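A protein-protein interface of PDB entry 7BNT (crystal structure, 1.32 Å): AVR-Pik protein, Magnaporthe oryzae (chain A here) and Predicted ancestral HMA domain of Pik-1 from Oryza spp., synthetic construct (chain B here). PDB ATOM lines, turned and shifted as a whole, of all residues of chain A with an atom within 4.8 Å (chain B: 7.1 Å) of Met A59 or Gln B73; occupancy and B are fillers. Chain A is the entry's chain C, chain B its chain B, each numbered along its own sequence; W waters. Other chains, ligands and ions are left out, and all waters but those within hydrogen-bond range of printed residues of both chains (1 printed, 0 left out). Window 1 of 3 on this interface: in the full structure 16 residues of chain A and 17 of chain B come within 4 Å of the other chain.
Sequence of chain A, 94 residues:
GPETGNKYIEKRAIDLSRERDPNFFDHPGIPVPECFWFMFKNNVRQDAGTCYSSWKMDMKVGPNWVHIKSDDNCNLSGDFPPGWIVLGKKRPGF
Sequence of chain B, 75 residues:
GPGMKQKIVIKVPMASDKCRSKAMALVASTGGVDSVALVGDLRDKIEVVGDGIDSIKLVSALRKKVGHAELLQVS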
ATOM      1  N   TRP A  37     -12.131 -36.898  12.389  1.00  0.00           N
ATOM      2  CA  TRP A  37     -11.984 -35.516  11.887  1.00  0.00           C
ATOM      3  C   TRP A  37     -10.505 -35.216  11.728  1.00  0.00           C
ATOM      4  O   TRP A  37      -9.665 -35.759  12.462  1.00  0.00           O
ATOM      5  CB  TRP A  37     -12.671 -34.479  12.777  1.00  0.00           C
ATOM      6  CG  TRP A  37     -12.150 -34.442  14.178  1.00  0.00           C
ATOM      7  CD1 TRP A  37     -12.646 -35.114  15.260  1.00  0.00           C
ATOM      8  CD2 TRP A  37     -10.999 -33.715  14.661  1.00  0.00           C
ATOM      9  NE1 TRP A  37     -11.908 -34.868  16.385  1.00  0.00           N
ATOM     10  CE2 TRP A  37     -10.889 -33.995  16.039  1.00  0.00           C
ATOM     11  CE3 TRP A  37     -10.038 -32.890  14.071  1.00  0.00           C
ATOM     12  CZ2 TRP A  37      -9.859 -33.489  16.813  1.00  0.00           C
ATOM     13  CZ3 TRP A  37      -9.026 -32.367  14.859  1.00  0.00           C
ATOM     14  CH2 TRP A  37      -8.935 -32.671  16.217  1.00  0.00           C
ATOM     15  N   MET A  39      -7.949 -31.723  10.986  1.00  0.00           N
ATOM     16  CA  MET A  39      -7.856 -30.247  10.926  1.00  0.00           C
ATOM     17  C   MET A  39      -6.622 -29.870  10.109  1.00  0.00           C
ATOM     18  O   MET A  39      -5.541 -30.438  10.337  1.00  0.00           O
ATOM     19  CB  MET A  39      -7.759 -29.676  12.345  1.00  0.00           C
ATOM     20  CG  MET A  39      -7.623 -28.153  12.359  1.00  0.00           C
ATOM     21  SD  MET A  39      -7.458 -27.516  14.042  1.00  0.00           S
ATOM     22  CE  MET A  39      -8.718 -28.330  14.983  1.00  0.00           C
ATOM     23  N   MET A  57     -20.032 -30.111  18.193  1.00  0.00           N
ATOM     24  CA  MET A  57     -18.953 -29.896  19.148  1.00  0.00           C
ATOM     25  C   MET A  57     -18.442 -28.476  18.995  1.00  0.00           C
ATOM     26  O   MET A  57     -18.641 -27.866  17.944  1.00  0.00           O
ATOM     27  CB  MET A  57     -17.832 -30.906  18.933  1.00  0.00           C
ATOM     28  CG  MET A  57     -17.224 -30.847  17.566  1.00  0.00           C
ATOM     29  SD  MET A  57     -15.944 -32.155  17.426  1.00  0.00           S
ATOM     30  CE  MET A  57     -15.700 -32.164  15.651  1.00  0.00           C
ATOM     31  N   ASP A  58     -17.812 -27.996  20.047  1.00  0.00           N
ATOM     32  CA  ASP A  58     -17.061 -26.737  19.987  1.00  0.00           C
ATOM     33  C   ASP A  58     -15.585 -27.082  20.012  1.00  0.00           C
ATOM     34  O   ASP A  58     -15.170 -27.877  20.849  1.00  0.00           O
ATOM     35  CB  ASP A  58     -17.407 -25.821  21.133  1.00  0.00           C
ATOM     36  CG  ASP A  58     -18.796 -25.224  21.083  1.00  0.00           C
ATOM     37  OD1 ASP A  58     -19.387 -25.133  19.981  1.00  0.00           O
ATOM     38  OD2 ASP A  58     -19.248 -24.818  22.152  1.00  0.00           O
ATOM     39  N   MET A  59     -14.850 -26.505  19.079  1.00  0.00           N
ATOM     40  CA  MET A  59     -13.429 -26.835  18.930  1.00  0.00           C
ATOM     41  C   MET A  59     -12.644 -25.577  18.634  1.00  0.00           C
ATOM     42  O   MET A  59     -13.091 -24.724  17.867  1.00  0.00           O
ATOM     43  CB  MET A  59     -13.263 -27.807  17.771  1.00  0.00           C
ATOM     44  CG  MET A  59     -11.862 -28.276  17.595  1.00  0.00           C
ATOM     45  SD  MET A  59     -11.678 -29.454  16.168  1.00  0.00           S
ATOM     46  CE  MET A  59     -12.572 -30.902  16.720  1.00  0.00           C
ATOM     47  N   LYS A  60     -11.455 -25.512  19.214  1.00  0.00           N
ATOM     48  CA  LYS A  60     -10.524 -24.424  18.905  1.00  0.00           C
ATOM     49  C   LYS A  60      -9.847 -24.731  17.571  1.00  0.00           C
ATOM     50  O   LYS A  60      -9.198 -25.764  17.445  1.00  0.00           O
ATOM     51  CB  LYS A  60      -9.528 -24.240  20.044  1.00  0.00           C
ATOM     52  CG  LYS A  60      -8.769 -22.931  19.964  1.00  0.00           C
ATOM     53  CD  LYS A  60      -9.614 -21.721  20.257  1.00  0.00           C
ATOM     54  CE  LYS A  60      -8.838 -20.433  20.105  1.00  0.00           C
ATOM     55  NZ  LYS A  60      -7.625 -20.420  20.951  1.00  0.00           N
ATOM     56  N   VAL A  61     -10.069 -23.869  16.588  1.00  0.00           N
ATOM     57  CA  VAL A  61      -9.514 -24.014  15.231  1.00  0.00           C
ATOM     58  C   VAL A  61      -8.681 -22.756  14.965  1.00  0.00           C
ATOM     59  O   VAL A  61      -9.229 -21.680  14.791  1.00  0.00           O
ATOM     60  CB  VAL A  61     -10.618 -24.207  14.183  1.00  0.00           C
ATOM     61  CG1 VAL A  61     -10.006 -24.383  12.813  1.00  0.00           C
ATOM     62  CG2 VAL A  61     -11.532 -25.370  14.523  1.00  0.00           C
ATOM     63  N   ASN A  64      -9.756 -19.261  16.726  1.00  0.00           N
ATOM     64  CA  ASN A  64     -11.186 -19.126  17.067  1.00  0.00           C
ATOM     65  C   ASN A  64     -11.790 -20.398  17.637  1.00  0.00           C
ATOM     66  O   ASN A  64     -11.428 -21.493  17.242  1.00  0.00           O
ATOM     67  CB  ASN A  64     -12.010 -18.738  15.860  1.00  0.00           C
ATOM     68  CG  ASN A  64     -11.671 -17.361  15.353  1.00  0.00           C
ATOM     69  OD1 ASN A  64     -10.990 -16.561  16.020  1.00  0.00           O
ATOM     70  ND2 ASN A  64     -12.126 -17.104  14.157  1.00  0.00           N
ATOM     71  N   TRP A  65     -12.723 -20.209  18.546  1.00  0.00           N
ATOM     72  CA  TRP A  65     -13.674 -21.264  18.917  1.00  0.00           C
ATOM     73  C   TRP A  65     -14.713 -21.402  17.817  1.00  0.00           C
ATOM     74  O   TRP A  65     -15.355 -20.390  17.468  1.00  0.00           O
ATOM     75  CB  TRP A  65     -14.395 -20.895  20.188  1.00  0.00           C
ATOM     76  CG  TRP A  65     -13.616 -21.261  21.368  1.00  0.00           C
ATOM     77  CD1 TRP A  65     -12.918 -20.416  22.175  1.00  0.00           C
ATOM     78  CD2 TRP A  65     -13.386 -22.594  21.860  1.00  0.00           C
ATOM     79  NE1 TRP A  65     -12.254 -21.130  23.137  1.00  0.00           N
ATOM     80  CE2 TRP A  65     -12.539 -22.459  22.984  1.00  0.00           C
ATOM     81  CE3 TRP A  65     -13.800 -23.850  21.471  1.00  0.00           C
ATOM     82  CZ2 TRP A  65     -12.103 -23.578  23.698  1.00  0.00           C
ATOM     83  CZ3 TRP A  65     -13.370 -24.943  22.179  1.00  0.00           C
ATOM     84  CH2 TRP A  65     -12.523 -24.813  23.254  1.00  0.00           C
ATOM     85  N   VAL A  66     -14.887 -22.617  17.321  1.00  0.00           N
ATOM     86  CA  VAL A  66     -15.794 -22.891  16.184  1.00  0.00           C
ATOM     87  C   VAL A  66     -16.799 -23.963  16.574  1.00  0.00           C
ATOM     88  O   VAL A  66     -16.410 -25.018  17.121  1.00  0.00           O
ATOM     89  CB  VAL A  66     -15.047 -23.367  14.938  1.00  0.00           C
ATOM     90  CG1 VAL A  66     -16.036 -23.585  13.793  1.00  0.00           C
ATOM     91  CG2 VAL A  66     -13.968 -22.376  14.522  1.00  0.00           C
ATOM     92  N   ILE A  68     -18.948 -26.803  15.408  1.00  0.00           N
ATOM     93  CA  ILE A  68     -18.859 -27.737  14.260  1.00  0.00           C
ATOM     94  C   ILE A  68     -20.013 -28.719  14.371  1.00  0.00           C
ATOM     95  O   ILE A  68     -20.106 -29.430  15.391  1.00  0.00           O
ATOM     96  CB  ILE A  68     -17.508 -28.463  14.232  1.00  0.00           C
ATOM     97  CG1 ILE A  68     -16.356 -27.456  14.189  1.00  0.00           C
ATOM     98  CG2 ILE A  68     -17.490 -29.416  13.058  1.00  0.00           C
ATOM     99  CD1 ILE A  68     -14.976 -28.083  14.216  1.00  0.00           C
ATOM    100  N   VAL A  86     -11.761 -28.107   8.979  1.00  0.00           N
ATOM    101  CA  VAL A  86     -11.902 -29.410   9.661  1.00  0.00           C
ATOM    102  C   VAL A  86     -12.820 -30.264   8.796  1.00  0.00           C
ATOM    103  O   VAL A  86     -13.901 -29.793   8.440  1.00  0.00           O
ATOM    104  CB  VAL A  86     -12.413 -29.279  11.101  1.00  0.00           C
ATOM    105  CG1 VAL A  86     -12.391 -30.635  11.763  1.00  0.00           C
ATOM    106  CG2 VAL A  86     -11.581 -28.286  11.902  1.00  0.00           C
ATOM    107  N   LYS B   7     -17.427 -34.745  27.250  1.00  0.00           N
ATOM    108  CA  LYS B   7     -16.065 -35.025  26.760  1.00  0.00           C
ATOM    109  C   LYS B   7     -15.413 -33.675  26.520  1.00  0.00           C
ATOM    110  O   LYS B   7     -15.994 -32.829  25.839  1.00  0.00           O
ATOM    111  CB  LYS B   7     -16.021 -35.863  25.478  1.00  0.00           C
ATOM    112  CG  LYS B   7     -14.606 -36.135  24.974  1.00  0.00           C
ATOM    113  CD  LYS B   7     -14.546 -37.071  23.775  1.00  0.00           C
ATOM    114  CE  LYS B   7     -15.587 -36.734  22.738  1.00  0.00           C
ATOM    115  NZ  LYS B   7     -15.444 -37.546  21.510  1.00  0.00           N
ATOM    116  N   ILE B   8     -14.245 -33.481  27.095  1.00  0.00           N
ATOM    117  CA  ILE B   8     -13.449 -32.282  26.768  1.00  0.00           C
ATOM    118  C   ILE B   8     -12.023 -32.724  26.465  1.00  0.00           C
ATOM    119  O   ILE B   8     -11.581 -33.826  26.844  1.00  0.00           O
ATOM    120  CB  ILE B   8     -13.487 -31.246  27.899  1.00  0.00           C
ATOM    121  CG1 ILE B   8     -12.805 -31.815  29.136  1.00  0.00           C
ATOM    122  CG2 ILE B   8     -14.904 -30.748  28.184  1.00  0.00           C
ATOM    123  CD1 ILE B   8     -12.674 -30.828  30.243  1.00  0.00           C
ATOM    124  N   VAL B   9     -11.333 -31.825  25.797  1.00  0.00           N
ATOM    125  CA  VAL B   9      -9.921 -32.024  25.397  1.00  0.00           C
ATOM    126  C   VAL B   9      -9.137 -30.794  25.844  1.00  0.00           C
ATOM    127  O   VAL B   9      -9.528 -29.668  25.510  1.00  0.00           O
ATOM    128  CB  VAL B   9      -9.775 -32.242  23.891  1.00  0.00           C
ATOM    129  CG1 VAL B   9      -8.321 -32.461  23.538  1.00  0.00           C
ATOM    130  CG2 VAL B   9     -10.620 -33.421  23.437  1.00  0.00           C
ATOM    131  N   ILE B  10      -8.058 -31.036  26.567  1.00  0.00           N
ATOM    132  CA  ILE B  10      -7.171 -29.984  27.101  1.00  0.00           C
ATOM    133  C   ILE B  10      -5.744 -30.256  26.625  1.00  0.00           C
ATOM    134  O   ILE B  10      -5.229 -31.360  26.820  1.00  0.00           O
ATOM    135  CB  ILE B  10      -7.262 -29.886  28.640  1.00  0.00           C
ATOM    136  CG1 ILE B  10      -8.671 -29.482  29.078  1.00  0.00           C
ATOM    137  CG2 ILE B  10      -6.228 -28.904  29.158  1.00  0.00           C
ATOM    138  CD1 ILE B  10      -8.927 -29.641  30.571  1.00  0.00           C
ATOM    139  N   LYS B  11      -5.129 -29.261  26.006  1.00  0.00           N
ATOM    140  CA  LYS B  11      -3.702 -29.324  25.629  1.00  0.00           C
ATOM    141  C   LYS B  11      -2.866 -29.102  26.890  1.00  0.00           C
ATOM    142  O   LYS B  11      -3.165 -28.166  27.669  1.00  0.00           O
ATOM    143  CB  LYS B  11      -3.356 -28.271  24.577  1.00  0.00           C
ATOM    144  CG  LYS B  11      -1.913 -28.351  24.066  1.00  0.00           C
ATOM    145  CD  LYS B  11      -1.717 -27.552  22.781  1.00  0.00           C
ATOM    146  CE  LYS B  11      -0.303 -27.532  22.252  1.00  0.00           C
ATOM    147  NZ  LYS B  11      -0.204 -26.738  21.000  1.00  0.00           N
ATOM    148  N   GLU B  47      -7.815 -36.095  26.667  1.00  0.00           N
ATOM    149  CA  GLU B  47      -9.274 -36.206  26.477  1.00  0.00           C
ATOM    150  C   GLU B  47      -9.866 -36.819  27.736  1.00  0.00           C
ATOM    151  O   GLU B  47      -9.439 -37.909  28.142  1.00  0.00           O
ATOM    152  CB  GLU B  47      -9.533 -37.080  25.275  1.00  0.00           C
ATOM    153  CG  GLU B  47     -10.945 -37.106  24.802  1.00  0.00           C
ATOM    154  CD  GLU B  47     -10.952 -37.883  23.480  1.00  0.00           C
ATOM    155  OE1 GLU B  47     -11.031 -39.121  23.506  1.00  0.00           O
ATOM    156  OE2 GLU B  47     -10.769 -37.256  22.403  1.00  0.00           O
ATOM    157  N   SER B  55     -14.712 -27.687  33.278  1.00  0.00           N
ATOM    158  CA  SER B  55     -13.578 -27.632  32.331  1.00  0.00           C
ATOM    159  C   SER B  55     -12.687 -26.440  32.678  1.00  0.00           C
ATOM    160  O   SER B  55     -11.455 -26.550  32.564  1.00  0.00           O
ATOM    161  CB  SER B  55     -14.067 -27.551  30.908  1.00  0.00           C
ATOM    162  OG  SER B  55     -14.870 -26.404  30.728  1.00  0.00           O
ATOM    163  N   GLU B  70      -4.654 -25.520  27.981  1.00  0.00           N
ATOM    164  CA  GLU B  70      -5.551 -24.813  27.052  1.00  0.00           C
ATOM    165  C   GLU B  70      -6.710 -25.739  26.692  1.00  0.00           C
ATOM    166  O   GLU B  70      -6.481 -26.834  26.177  1.00  0.00           O
ATOM    167  CB  GLU B  70      -4.744 -24.383  25.822  1.00  0.00           C
ATOM    168  CG  GLU B  70      -5.525 -23.615  24.802  1.00  0.00           C
ATOM    169  CD  GLU B  70      -4.686 -23.197  23.600  1.00  0.00           C
ATOM    170  OE1 GLU B  70      -3.515 -23.673  23.473  1.00  0.00           O
ATOM    171  OE2 GLU B  70      -5.210 -22.435  22.768  1.00  0.00           O
ATOM    172  N   LEU B  71      -7.923 -25.297  26.959  1.00  0.00           N
ATOM    173  CA  LEU B  71      -9.130 -26.022  26.514  1.00  0.00           C
ATOM    174  C   LEU B  71      -9.214 -25.973  24.997  1.00  0.00           C
ATOM    175  O   LEU B  71      -9.194 -24.863  24.435  1.00  0.00           O
ATOM    176  CB  LEU B  71     -10.361 -25.411  27.160  1.00  0.00           C
ATOM    177  CG  LEU B  71     -11.706 -26.071  26.877  1.00  0.00           C
ATOM    178  CD1 LEU B  71     -11.739 -27.500  27.370  1.00  0.00           C
ATOM    179  CD2 LEU B  71     -12.820 -25.280  27.524  1.00  0.00           C
ATOM    180  N   LEU B  72      -9.403 -27.127  24.359  1.00  0.00           N
ATOM    181  CA  LEU B  72      -9.468 -27.141  22.889  1.00  0.00           C
ATOM    182  C   LEU B  72     -10.759 -27.732  22.350  1.00  0.00           C
ATOM    183  O   LEU B  72     -11.011 -27.534  21.155  1.00  0.00           O
ATOM    184  CB  LEU B  72      -8.271 -27.899  22.311  1.00  0.00           C
ATOM    185  CG  LEU B  72      -6.897 -27.289  22.570  1.00  0.00           C
ATOM    186  CD1 LEU B  72      -5.865 -28.137  21.862  1.00  0.00           C
ATOM    187  CD2 LEU B  72      -6.787 -25.852  22.100  1.00  0.00           C
ATOM    188  N   GLN B  73     -11.507 -28.507  23.136  1.00  0.00           N
ATOM    189  CA  GLN B  73     -12.740 -29.098  22.591  1.00  0.00           C
ATOM    190  C   GLN B  73     -13.700 -29.359  23.740  1.00  0.00           C
ATOM    191  O   GLN B  73     -13.248 -29.808  24.797  1.00  0.00           O
ATOM    192  CB  GLN B  73     -12.437 -30.417  21.877  1.00  0.00           C
ATOM    193  CG  GLN B  73     -13.600 -30.955  21.060  1.00  0.00           C
ATOM    194  CD  GLN B  73     -13.382 -32.358  20.557  1.00  0.00           C
ATOM    195  OE1 GLN B  73     -12.375 -32.667  19.928  1.00  0.00           O
ATOM    196  NE2 GLN B  73     -14.368 -33.190  20.796  1.00  0.00           N
ATOM    197  N   VAL B  74     -14.981 -29.121  23.466  1.00  0.00           N
ATOM    198  CA  VAL B  74     -16.100 -29.526  24.349  1.00  0.00           C
ATOM    199  C   VAL B  74     -17.125 -30.205  23.453  1.00  0.00           C
ATOM    200  O   VAL B  74     -17.552 -29.613  22.441  1.00  0.00           O
ATOM    201  CB  VAL B  74     -16.691 -28.299  25.062  1.00  0.00           C
ATOM    202  CG1 VAL B  74     -17.859 -28.685  25.941  1.00  0.00           C
ATOM    203  CG2 VAL B  74     -15.632 -27.559  25.864  1.00  0.00           C
ATOM    204  N   SER B  75     -17.528 -31.407  23.819  1.00  0.00           N
ATOM    205  CA  SER B  75     -18.526 -32.138  23.021  1.00  0.00           C
ATOM    206  C   SER B  75     -19.375 -33.037  23.908  1.00  0.00           C
ATOM    207  O   SER B  75     -19.080 -33.235  25.073  1.00  0.00           O
ATOM    208  CB  SER B  75     -17.852 -32.867  21.934  1.00  0.00           C
ATOM    209  OG  SER B  75     -16.939 -33.804  22.430  1.00  0.00           O
ATOM    210  OXT SER B  75     -20.413 -33.503  23.372  1.00  0.00           O
HETATM  211  O   HOH W   1     -11.723 -35.450  19.236  1.00  0.00           O
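SD of Met A57 touches NE2 of Gln B73, at 3.9 Å.
O of Val B74 touches CA of Met A57, at 3.6 Å.
CB of Met A57 touches CB of Ser B75, at 3.6 Å.
CA of Gln B73 touches O of Asp A58, 3.2 Å away.
Met A59 touches Leu B72 (CA to O, 3.4 Å).
CE of Met A59 touches OE1 of Gln B73 (3.7 Å).
Leu B71 touches Trp A65.
Leu B72 touches Trp A65.
Trp A65 touches Gln B73 (CH2 to N, 3.8 Å).
NZ of Lys A60 is in salt-bridge range of OE2 of Glu B70 (3.6 Å).
O of Leu B72 lies within hydrogen-bond range of N of Lys A60 (2.8 Å).
N of Asp A58 lies within hydrogen-bond range of O of Val B74 (2.9 Å).
Water W1 lies within hydrogen-bond range of NE1 of Trp A37 (2.9 Å) and OE1 of Gln B73 (2.9 Å).
The backbone carbonyl oxygen (O) of Val B9 lies within hydrogen-bond range of the backbone NH (N) of Leu B72, at 2.8 Å.
The backbone NH (N) of Val B9 sits at hydrogen-bond distance from the backbone carbonyl oxygen (O) of Gln B73, at 3.0 Å.
The backbone NH (N) of Lys B11 sits at hydrogen-bond distance from the backbone carbonyl oxygen (O) of Glu B70, at 2.8 Å.
OG of Ser B75 is in hydrogen-bond range of NE2 of Gln B73 (3.1 Å).
O of Met A57 lies within hydrogen-bond range of N of Ile A68 (2.8 Å).
The backbone carbonyl oxygen (O) of Met A59 sits at hydrogen-bond distance from the backbone NH (N) of Val A66.
Printed residues of chain B that touch a printed residue of chain A: Glu B70, Leu B71, Leu B72, Gln B73, Val B74 and Ser B75.
Hydrophobic or aromatic side chains of chain B that line the printed part of chain A: Leu B71 and Leu B72.
Among the printed residues, 12 pairs touch across the chains.
Among the printed residues, Asp or Glu carboxylates within 4 Å of a Lys or Arg side-chain nitrogen of the other chain: Lys A60 with Glu B70 (3.6 Å).
Of the printed residues of chain B, Met A57 touches Gln B73, Val B74 and Ser B75.
Of chain B, only Leu B72 (3.4 Å) and Gln B73 (3.7 Å) come within 4 Å of Met A59.
Of the printed residues of chain B, Lys A60 touches Glu B70 and Leu B72.
Ile B8 touches none of the printed residues of chain A.
Glu B47 touches none of the printed residues of chain A.
Printed residues of chain A within 4 Å of Glu B70: Lys A60.
Of the printed residues of chain A, Leu B71 touches Trp A65 (3.3 Å).
Of chain A, only Met A57, Asp A58, Met A59 and Trp A65 come within 4 Å of Gln B73.
Of the printed residues of chain A, Val B74 touches Met A57 (3.6 Å) and Asp A58 (2.9 Å).
The nearest residue of chain B that does not touch Met A59 is Val B74 (5.1 Å).
The nearest residue of chain A that does not touch Gln B73 is Trp A37 (4.1 Å).
The nearest printed residue of chain B that does not touch Asp A58 is Leu B72 (4.2 Å).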
